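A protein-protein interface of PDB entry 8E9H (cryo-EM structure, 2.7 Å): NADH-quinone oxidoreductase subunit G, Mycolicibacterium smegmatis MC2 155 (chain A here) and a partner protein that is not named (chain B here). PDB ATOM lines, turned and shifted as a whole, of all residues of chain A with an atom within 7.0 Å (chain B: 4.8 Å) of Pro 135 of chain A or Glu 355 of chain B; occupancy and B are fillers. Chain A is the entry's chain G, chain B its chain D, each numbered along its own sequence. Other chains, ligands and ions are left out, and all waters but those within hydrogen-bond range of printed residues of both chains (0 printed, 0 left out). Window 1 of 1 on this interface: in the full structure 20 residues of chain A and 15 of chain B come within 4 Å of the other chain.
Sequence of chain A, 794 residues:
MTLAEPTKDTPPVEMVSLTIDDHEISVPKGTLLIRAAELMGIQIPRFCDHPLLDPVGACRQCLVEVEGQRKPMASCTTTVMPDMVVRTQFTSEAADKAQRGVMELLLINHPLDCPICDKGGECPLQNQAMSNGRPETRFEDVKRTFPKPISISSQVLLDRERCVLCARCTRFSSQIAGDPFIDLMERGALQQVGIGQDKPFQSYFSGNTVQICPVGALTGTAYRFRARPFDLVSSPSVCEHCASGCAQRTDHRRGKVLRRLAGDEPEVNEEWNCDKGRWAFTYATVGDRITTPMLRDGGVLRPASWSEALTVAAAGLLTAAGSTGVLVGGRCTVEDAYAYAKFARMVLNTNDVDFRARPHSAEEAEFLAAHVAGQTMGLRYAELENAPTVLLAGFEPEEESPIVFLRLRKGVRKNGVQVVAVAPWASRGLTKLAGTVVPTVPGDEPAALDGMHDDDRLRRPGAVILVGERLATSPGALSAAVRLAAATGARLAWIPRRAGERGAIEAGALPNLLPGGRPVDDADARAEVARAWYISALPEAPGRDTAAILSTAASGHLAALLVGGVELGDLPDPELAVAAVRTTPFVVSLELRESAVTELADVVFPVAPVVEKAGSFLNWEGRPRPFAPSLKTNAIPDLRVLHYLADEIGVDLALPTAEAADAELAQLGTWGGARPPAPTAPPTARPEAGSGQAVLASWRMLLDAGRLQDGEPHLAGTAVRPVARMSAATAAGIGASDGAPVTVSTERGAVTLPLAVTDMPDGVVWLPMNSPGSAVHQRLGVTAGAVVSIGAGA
The side-chain amino group (NZ) of Lys 325 of chain B sits at hydrogen-bond distance from the backbone carbonyl oxygen (O) of Ala 129 of chain A. NZ of Lys 325 of chain B is in hydrogen-bond range of O of Met 130 of chain A, 2.6 Å away. NZ of Lys 325 of chain B sits at hydrogen-bond distance from O of Gly 133 of chain A, at 2.6 Å. OG1 of Thr 137 of chain A lies within hydrogen-bond range of OG of Ser 353 of chain B (3.3 Å). NE2 of His 359 of chain B sits close to SD of Met 130 of chain A (3.5 Å).
The side-chain amino group (NZ) of Lys 325 of chain B lies within hydrogen-bond range of a ring nitrogen (NE2) of His 359 of chain B, at 3.2 Å. OG of Ser 353 of chain B lies within hydrogen-bond range of N of Gly 356 of chain B, at 2.8 Å. ND1 of His 359 of chain B lies within hydrogen-bond range of O of Glu 355 of chain B. The guanidinium group of Arg 100 of chain A sits at hydrogen-bond distance from the backbone carbonyl oxygen of Gly 133 of chain A, 2.8 Å away. NH1 of Arg 134 of chain A is in salt-bridge range of OE2 of Glu 104 of chain A, at 3.8 Å. The side-chain amino group (NZ) of Lys 143 of chain A sits at hydrogen-bond distance from the backbone carbonyl oxygen (O) of Ile 108 of chain A.
CD1 of Leu 107 of chain A touches CD of Glu 355 of chain B, 3.4 Å away. Leu 107 of chain A touches Ile 358 of chain B. Leu 112 of chain A touches Ser 353 of chain B (CD2 to O, 3.9 Å). Leu 112 of chain A touches Met 354 of chain B (CD1 to CA, 3.97 Å). Ile 358 of chain B touches Ala 129 of chain A (CD1 to CB, 3.8 Å). Arg 134 of chain A touches Glu 355 of chain B. Lys 324 of chain B touches Pro 135 of chain A. Pro 135 of chain A touches His 359 of chain B. Glu 355 of chain B touches Thr 137 of chain A (OE1 to CG2, 2.8 Å). Met 354 of chain B touches Lys 143 of chain A.
Of the printed residues of chain B, Pro 135 of chain A touches Lys 324 (3.4 Å), Glu 355 (3.6 Å) and His 359 (3.6 Å). Of chain A, only Leu 107 (3.4 Å), Arg 134 (3.3 Å), Pro 135 (3.6 Å), Glu 136 (3.9 Å) and Thr 137 (2.8 Å) come within 4 Å of Glu 355 of chain B. Of the printed residues of chain B, Lys 143 of chain A touches Met 354. Of the printed residues of chain B, Glu 136 of chain A touches Glu 355. Leu 105 of chain A touches none of the printed residues of chain B. Glu 104 of chain A touches none of the printed residues of chain B. The nearest printed residue of chain B that does not touch Pro 135 of chain A is Gly 356 of chain B (4.01 Å). The nearest printed residue of chain A that does not touch Lys 325 of chain B is Arg 134 of chain A (4.04 Å).
Among the printed residues, no Asp or Glu carboxylate lies within 4 Å of a Lys or Arg side-chain nitrogen of the other chain.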
ATOM      1  N   ARG A 100      -7.117 -33.221 -20.084  1.00  0.00           N
ATOM      2  CA  ARG A 100      -7.384 -32.324 -18.967  1.00  0.00           C
ATOM      3  C   ARG A 100      -7.074 -30.881 -19.330  1.00  0.00           C
ATOM      4  O   ARG A 100      -7.786 -29.966 -18.909  1.00  0.00           O
ATOM      5  CB  ARG A 100      -6.587 -32.760 -17.746  1.00  0.00           C
ATOM      6  CG  ARG A 100      -7.192 -33.959 -17.066  1.00  0.00           C
ATOM      7  CD  ARG A 100      -6.326 -34.478 -15.949  1.00  0.00           C
ATOM      8  NE  ARG A 100      -6.842 -35.747 -15.456  1.00  0.00           N
ATOM      9  CZ  ARG A 100      -7.878 -35.860 -14.639  1.00  0.00           C
ATOM     10  NH1 ARG A 100      -8.520 -34.797 -14.185  1.00  0.00           N
ATOM     11  NH2 ARG A 100      -8.284 -37.071 -14.271  1.00  0.00           N
ATOM     12  N   MET A 103     -10.013 -29.746 -21.298  1.00  0.00           N
ATOM     13  CA  MET A 103     -11.139 -29.457 -20.416  1.00  0.00           C
ATOM     14  C   MET A 103     -10.949 -28.124 -19.707  1.00  0.00           C
ATOM     15  O   MET A 103     -11.887 -27.322 -19.609  1.00  0.00           O
ATOM     16  CB  MET A 103     -11.308 -30.582 -19.400  1.00  0.00           C
ATOM     17  CG  MET A 103     -12.440 -30.368 -18.413  1.00  0.00           C
ATOM     18  SD  MET A 103     -14.043 -30.221 -19.208  1.00  0.00           S
ATOM     19  CE  MET A 103     -14.216 -31.857 -19.901  1.00  0.00           C
ATOM     20  N   GLU A 104      -9.742 -27.868 -19.206  1.00  0.00           N
ATOM     21  CA  GLU A 104      -9.465 -26.589 -18.566  1.00  0.00           C
ATOM     22  C   GLU A 104      -9.739 -25.439 -19.521  1.00  0.00           C
ATOM     23  O   GLU A 104     -10.473 -24.503 -19.190  1.00  0.00           O
ATOM     24  CB  GLU A 104      -8.016 -26.555 -18.083  1.00  0.00           C
ATOM     25  CG  GLU A 104      -7.557 -25.203 -17.574  1.00  0.00           C
ATOM     26  CD  GLU A 104      -6.109 -25.211 -17.143  1.00  0.00           C
ATOM     27  OE1 GLU A 104      -5.299 -25.898 -17.798  1.00  0.00           O
ATOM     28  OE2 GLU A 104      -5.775 -24.524 -16.155  1.00  0.00           O
ATOM     29  N   LEU A 105      -9.167 -25.500 -20.724  1.00  0.00           N
ATOM     30  CA  LEU A 105      -9.402 -24.441 -21.699  1.00  0.00           C
ATOM     31  C   LEU A 105     -10.876 -24.331 -22.047  1.00  0.00           C
ATOM     32  O   LEU A 105     -11.349 -23.258 -22.431  1.00  0.00           O
ATOM     33  CB  LEU A 105      -8.582 -24.700 -22.958  1.00  0.00           C
ATOM     34  CG  LEU A 105      -7.070 -24.632 -22.772  1.00  0.00           C
ATOM     35  CD1 LEU A 105      -6.370 -25.021 -24.050  1.00  0.00           C
ATOM     36  CD2 LEU A 105      -6.644 -23.248 -22.336  1.00  0.00           C
ATOM     37  N   LEU A 107     -13.298 -24.755 -19.851  1.00  0.00           N
ATOM     38  CA  LEU A 107     -14.025 -24.210 -18.714  1.00  0.00           C
ATOM     39  C   LEU A 107     -13.652 -22.778 -18.369  1.00  0.00           C
ATOM     40  O   LEU A 107     -14.371 -22.145 -17.589  1.00  0.00           O
ATOM     41  CB  LEU A 107     -13.795 -25.077 -17.475  1.00  0.00           C
ATOM     42  CG  LEU A 107     -14.531 -26.411 -17.442  1.00  0.00           C
ATOM     43  CD1 LEU A 107     -14.100 -27.212 -16.236  1.00  0.00           C
ATOM     44  CD2 LEU A 107     -16.026 -26.198 -17.425  1.00  0.00           C
ATOM     45  N   ILE A 108     -12.557 -22.243 -18.908  1.00  0.00           N
ATOM     46  CA  ILE A 108     -12.114 -20.924 -18.465  1.00  0.00           C
ATOM     47  C   ILE A 108     -13.169 -19.873 -18.777  1.00  0.00           C
ATOM     48  O   ILE A 108     -13.495 -19.032 -17.932  1.00  0.00           O
ATOM     49  CB  ILE A 108     -10.754 -20.564 -19.090  1.00  0.00           C
ATOM     50  CG1 ILE A 108     -10.825 -20.579 -20.613  1.00  0.00           C
ATOM     51  CG2 ILE A 108      -9.686 -21.517 -18.606  1.00  0.00           C
ATOM     52  CD1 ILE A 108      -9.517 -20.245 -21.269  1.00  0.00           C
ATOM     53  N   LEU A 112     -20.374 -19.262 -14.608  1.00  0.00           N
ATOM     54  CA  LEU A 112     -20.660 -19.921 -13.337  1.00  0.00           C
ATOM     55  C   LEU A 112     -22.174 -20.043 -13.154  1.00  0.00           C
ATOM     56  O   LEU A 112     -22.772 -19.501 -12.228  1.00  0.00           O
ATOM     57  CB  LEU A 112     -20.017 -19.150 -12.193  1.00  0.00           C
ATOM     58  CG  LEU A 112     -18.547 -19.479 -11.941  1.00  0.00           C
ATOM     59  CD1 LEU A 112     -17.736 -19.277 -13.198  1.00  0.00           C
ATOM     60  CD2 LEU A 112     -17.997 -18.635 -10.815  1.00  0.00           C
ATOM     61  N   ALA A 129     -16.162 -32.832 -16.877  1.00  0.00           N
ATOM     62  CA  ALA A 129     -15.214 -32.066 -16.082  1.00  0.00           C
ATOM     63  C   ALA A 129     -14.916 -32.767 -14.770  1.00  0.00           C
ATOM     64  O   ALA A 129     -13.776 -32.745 -14.299  1.00  0.00           O
ATOM     65  CB  ALA A 129     -15.755 -30.666 -15.818  1.00  0.00           C
ATOM     66  N   MET A 130     -15.925 -33.393 -14.169  1.00  0.00           N
ATOM     67  CA  MET A 130     -15.688 -34.191 -12.974  1.00  0.00           C
ATOM     68  C   MET A 130     -14.771 -35.365 -13.283  1.00  0.00           C
ATOM     69  O   MET A 130     -13.792 -35.613 -12.571  1.00  0.00           O
ATOM     70  CB  MET A 130     -17.020 -34.685 -12.414  1.00  0.00           C
ATOM     71  CG  MET A 130     -17.806 -33.648 -11.641  1.00  0.00           C
ATOM     72  SD  MET A 130     -16.846 -32.861 -10.344  1.00  0.00           S
ATOM     73  CE  MET A 130     -17.288 -33.893  -8.955  1.00  0.00           C
ATOM     74  N   GLY A 133     -11.452 -33.602 -15.563  1.00  0.00           N
ATOM     75  CA  GLY A 133     -11.051 -32.223 -15.394  1.00  0.00           C
ATOM     76  C   GLY A 133     -10.285 -31.999 -14.112  1.00  0.00           C
ATOM     77  O   GLY A 133     -10.262 -32.863 -13.234  1.00  0.00           O
ATOM     78  N   ARG A 134      -9.648 -30.842 -13.996  1.00  0.00           N
ATOM     79  CA  ARG A 134      -8.937 -30.505 -12.782  1.00  0.00           C
ATOM     80  C   ARG A 134      -9.925 -30.101 -11.693  1.00  0.00           C
ATOM     81  O   ARG A 134     -11.074 -29.764 -11.978  1.00  0.00           O
ATOM     82  CB  ARG A 134      -7.952 -29.379 -13.049  1.00  0.00           C
ATOM     83  CG  ARG A 134      -8.581 -28.097 -13.547  1.00  0.00           C
ATOM     84  CD  ARG A 134      -7.486 -27.119 -13.849  1.00  0.00           C
ATOM     85  NE  ARG A 134      -6.752 -26.792 -12.634  1.00  0.00           N
ATOM     86  CZ  ARG A 134      -5.432 -26.745 -12.536  1.00  0.00           C
ATOM     87  NH1 ARG A 134      -4.648 -27.056 -13.555  1.00  0.00           N
ATOM     88  NH2 ARG A 134      -4.881 -26.403 -11.375  1.00  0.00           N
ATOM     89  N   PRO A 135      -9.502 -30.134 -10.435  1.00  0.00           N
ATOM     90  CA  PRO A 135     -10.440 -29.849  -9.344  1.00  0.00           C
ATOM     91  C   PRO A 135     -10.720 -28.370  -9.131  1.00  0.00           C
ATOM     92  O   PRO A 135     -11.811 -28.011  -8.678  1.00  0.00           O
ATOM     93  CB  PRO A 135      -9.741 -30.462  -8.128  1.00  0.00           C
ATOM     94  CG  PRO A 135      -8.309 -30.370  -8.450  1.00  0.00           C
ATOM     95  CD  PRO A 135      -8.202 -30.597  -9.926  1.00  0.00           C
ATOM     96  N   GLU A 136      -9.760 -27.502  -9.443  1.00  0.00           N
ATOM     97  CA  GLU A 136      -9.925 -26.077  -9.197  1.00  0.00           C
ATOM     98  C   GLU A 136      -9.341 -25.291 -10.360  1.00  0.00           C
ATOM     99  O   GLU A 136      -8.480 -25.779 -11.096  1.00  0.00           O
ATOM    100  CB  GLU A 136      -9.262 -25.655  -7.882  1.00  0.00           C
ATOM    101  N   THR A 137      -9.819 -24.060 -10.514  1.00  0.00           N
ATOM    102  CA  THR A 137      -9.412 -23.234 -11.642  1.00  0.00           C
ATOM    103  C   THR A 137      -8.022 -22.650 -11.439  1.00  0.00           C
ATOM    104  O   THR A 137      -7.538 -22.496 -10.316  1.00  0.00           O
ATOM    105  CB  THR A 137     -10.393 -22.085 -11.857  1.00  0.00           C
ATOM    106  OG1 THR A 137     -10.618 -21.408 -10.615  1.00  0.00           O
ATOM    107  CG2 THR A 137     -11.695 -22.584 -12.417  1.00  0.00           C
ATOM    108  N   ARG A 138      -7.384 -22.329 -12.560  1.00  0.00           N
ATOM    109  CA  ARG A 138      -6.237 -21.441 -12.602  1.00  0.00           C
ATOM    110  C   ARG A 138      -6.551 -20.127 -13.294  1.00  0.00           C
ATOM    111  O   ARG A 138      -5.695 -19.239 -13.319  1.00  0.00           O
ATOM    112  CB  ARG A 138      -5.069 -22.115 -13.326  1.00  0.00           C
ATOM    113  CG  ARG A 138      -4.357 -23.157 -12.507  1.00  0.00           C
ATOM    114  CD  ARG A 138      -3.761 -24.225 -13.392  1.00  0.00           C
ATOM    115  NE  ARG A 138      -2.583 -23.776 -14.118  1.00  0.00           N
ATOM    116  CZ  ARG A 138      -2.162 -24.303 -15.259  1.00  0.00           C
ATOM    117  NH1 ARG A 138      -2.826 -25.274 -15.861  1.00  0.00           N
ATOM    118  NH2 ARG A 138      -1.043 -23.845 -15.809  1.00  0.00           N
ATOM    119  N   PHE A 139      -7.749 -19.984 -13.850  1.00  0.00           N
ATOM    120  CA  PHE A 139      -8.120 -18.819 -14.648  1.00  0.00           C
ATOM    121  C   PHE A 139      -8.536 -17.691 -13.717  1.00  0.00           C
ATOM    122  O   PHE A 139      -9.694 -17.578 -13.317  1.00  0.00           O
ATOM    123  CB  PHE A 139      -9.239 -19.178 -15.613  1.00  0.00           C
ATOM    124  CG  PHE A 139      -9.565 -18.093 -16.584  1.00  0.00           C
ATOM    125  CD1 PHE A 139      -8.789 -17.898 -17.707  1.00  0.00           C
ATOM    126  CD2 PHE A 139     -10.653 -17.273 -16.380  1.00  0.00           C
ATOM    127  CE1 PHE A 139      -9.091 -16.907 -18.604  1.00  0.00           C
ATOM    128  CE2 PHE A 139     -10.957 -16.280 -17.275  1.00  0.00           C
ATOM    129  CZ  PHE A 139     -10.175 -16.096 -18.388  1.00  0.00           C
ATOM    130  N   LYS A 143     -13.542 -13.399 -17.931  1.00  0.00           N
ATOM    131  CA  LYS A 143     -14.227 -14.343 -18.799  1.00  0.00           C
ATOM    132  C   LYS A 143     -14.895 -13.630 -19.966  1.00  0.00           C
ATOM    133  O   LYS A 143     -15.333 -12.483 -19.848  1.00  0.00           O
ATOM    134  CB  LYS A 143     -15.280 -15.119 -18.016  1.00  0.00           C
ATOM    135  CG  LYS A 143     -14.717 -16.111 -17.030  1.00  0.00           C
ATOM    136  CD  LYS A 143     -15.825 -16.764 -16.235  1.00  0.00           C
ATOM    137  CE  LYS A 143     -15.270 -17.728 -15.215  1.00  0.00           C
ATOM    138  NZ  LYS A 143     -14.994 -19.058 -15.810  1.00  0.00           N
ATOM    139  N   LYS B 324     -10.445 -33.423  -4.132  1.00  0.00           N
ATOM    140  CA  LYS B 324     -11.647 -32.657  -4.432  1.00  0.00           C
ATOM    141  C   LYS B 324     -12.667 -33.472  -5.208  1.00  0.00           C
ATOM    142  O   LYS B 324     -13.858 -33.154  -5.165  1.00  0.00           O
ATOM    143  CB  LYS B 324     -11.286 -31.405  -5.221  1.00  0.00           C
ATOM    144  CG  LYS B 324     -10.390 -30.437  -4.477  1.00  0.00           C
ATOM    145  CD  LYS B 324     -11.119 -29.792  -3.317  1.00  0.00           C
ATOM    146  CE  LYS B 324     -10.236 -28.793  -2.602  1.00  0.00           C
ATOM    147  NZ  LYS B 324      -9.964 -27.601  -3.448  1.00  0.00           N
ATOM    148  N   LYS B 325     -12.232 -34.511  -5.918  1.00  0.00           N
ATOM    149  CA  LYS B 325     -13.170 -35.342  -6.657  1.00  0.00           C
ATOM    150  C   LYS B 325     -14.102 -36.114  -5.737  1.00  0.00           C
ATOM    151  O   LYS B 325     -15.125 -36.625  -6.202  1.00  0.00           O
ATOM    152  CB  LYS B 325     -12.412 -36.317  -7.552  1.00  0.00           C
ATOM    153  CG  LYS B 325     -11.532 -35.653  -8.589  1.00  0.00           C
ATOM    154  CD  LYS B 325     -12.357 -34.933  -9.635  1.00  0.00           C
ATOM    155  CE  LYS B 325     -11.478 -34.329 -10.707  1.00  0.00           C
ATOM    156  NZ  LYS B 325     -12.274 -33.618 -11.735  1.00  0.00           N
ATOM    157  N   SER B 353     -14.523 -19.713  -9.376  1.00  0.00           N
ATOM    158  CA  SER B 353     -14.078 -21.020  -9.848  1.00  0.00           C
ATOM    159  C   SER B 353     -15.211 -21.716 -10.591  1.00  0.00           C
ATOM    160  O   SER B 353     -16.252 -22.022 -10.005  1.00  0.00           O
ATOM    161  CB  SER B 353     -13.600 -21.873  -8.678  1.00  0.00           C
ATOM    162  OG  SER B 353     -13.063 -23.099  -9.134  1.00  0.00           O
ATOM    163  N   MET B 354     -15.003 -21.972 -11.882  1.00  0.00           N
ATOM    164  CA  MET B 354     -15.954 -22.780 -12.636  1.00  0.00           C
ATOM    165  C   MET B 354     -15.827 -24.249 -12.249  1.00  0.00           C
ATOM    166  O   MET B 354     -16.831 -24.940 -12.052  1.00  0.00           O
ATOM    167  CB  MET B 354     -15.716 -22.590 -14.132  1.00  0.00           C
ATOM    168  CG  MET B 354     -16.588 -23.434 -15.038  1.00  0.00           C
ATOM    169  SD  MET B 354     -18.264 -22.796 -15.129  1.00  0.00           S
ATOM    170  CE  MET B 354     -19.180 -24.063 -14.279  1.00  0.00           C
ATOM    171  N   GLU B 355     -14.592 -24.745 -12.139  1.00  0.00           N
ATOM    172  CA  GLU B 355     -14.388 -26.113 -11.681  1.00  0.00           C
ATOM    173  C   GLU B 355     -14.917 -26.301 -10.269  1.00  0.00           C
ATOM    174  O   GLU B 355     -15.511 -27.337  -9.954  1.00  0.00           O
ATOM    175  CB  GLU B 355     -12.906 -26.477 -11.730  1.00  0.00           C
ATOM    176  CG  GLU B 355     -12.412 -26.922 -13.087  1.00  0.00           C
ATOM    177  CD  GLU B 355     -12.050 -25.759 -13.975  1.00  0.00           C
ATOM    178  OE1 GLU B 355     -12.763 -24.739 -13.925  1.00  0.00           O
ATOM    179  OE2 GLU B 355     -11.053 -25.863 -14.717  1.00  0.00           O
ATOM    180  N   GLY B 356     -14.692 -25.321  -9.397  1.00  0.00           N
ATOM    181  CA  GLY B 356     -15.242 -25.411  -8.058  1.00  0.00           C
ATOM    182  C   GLY B 356     -16.753 -25.497  -8.070  1.00  0.00           C
ATOM    183  O   GLY B 356     -17.347 -26.276  -7.324  1.00  0.00           O
ATOM    184  N   LEU B 357     -17.395 -24.701  -8.922  1.00  0.00           N
ATOM    185  CA  LEU B 357     -18.846 -24.758  -9.025  1.00  0.00           C
ATOM    186  C   LEU B 357     -19.310 -26.112  -9.533  1.00  0.00           C
ATOM    187  O   LEU B 357     -20.275 -26.676  -9.007  1.00  0.00           O
ATOM    188  CB  LEU B 357     -19.347 -23.648  -9.943  1.00  0.00           C
ATOM    189  CG  LEU B 357     -20.859 -23.567 -10.130  1.00  0.00           C
ATOM    190  CD1 LEU B 357     -21.560 -23.401  -8.800  1.00  0.00           C
ATOM    191  CD2 LEU B 357     -21.188 -22.419 -11.051  1.00  0.00           C
ATOM    192  N   ILE B 358     -18.651 -26.647 -10.558  1.00  0.00           N
ATOM    193  CA  ILE B 358     -19.057 -27.945 -11.085  1.00  0.00           C
ATOM    194  C   ILE B 358     -18.917 -29.010 -10.011  1.00  0.00           C
ATOM    195  O   ILE B 358     -19.794 -29.861  -9.835  1.00  0.00           O
ATOM    196  CB  ILE B 358     -18.239 -28.306 -12.336  1.00  0.00           C
ATOM    197  CG1 ILE B 358     -18.680 -27.446 -13.517  1.00  0.00           C
ATOM    198  CG2 ILE B 358     -18.391 -29.783 -12.650  1.00  0.00           C
ATOM    199  CD1 ILE B 358     -17.852 -27.641 -14.764  1.00  0.00           C
ATOM    200  N   HIS B 359     -17.800 -28.989  -9.287  1.00  0.00           N
ATOM    201  CA  HIS B 359     -17.583 -29.985  -8.250  1.00  0.00           C
ATOM    202  C   HIS B 359     -18.616 -29.865  -7.146  1.00  0.00           C
ATOM    203  O   HIS B 359     -19.164 -30.873  -6.690  1.00  0.00           O
ATOM    204  CB  HIS B 359     -16.172 -29.852  -7.691  1.00  0.00           C
ATOM    205  CG  HIS B 359     -15.131 -30.477  -8.562  1.00  0.00           C
ATOM    206  ND1 HIS B 359     -14.759 -29.941  -9.774  1.00  0.00           N
ATOM    207  CD2 HIS B 359     -14.393 -31.598  -8.402  1.00  0.00           C
ATOM    208  CE1 HIS B 359     -13.833 -30.704 -10.324  1.00  0.00           C
ATOM    209  NE2 HIS B 359     -13.592 -31.715  -9.511  1.00  0.00           N
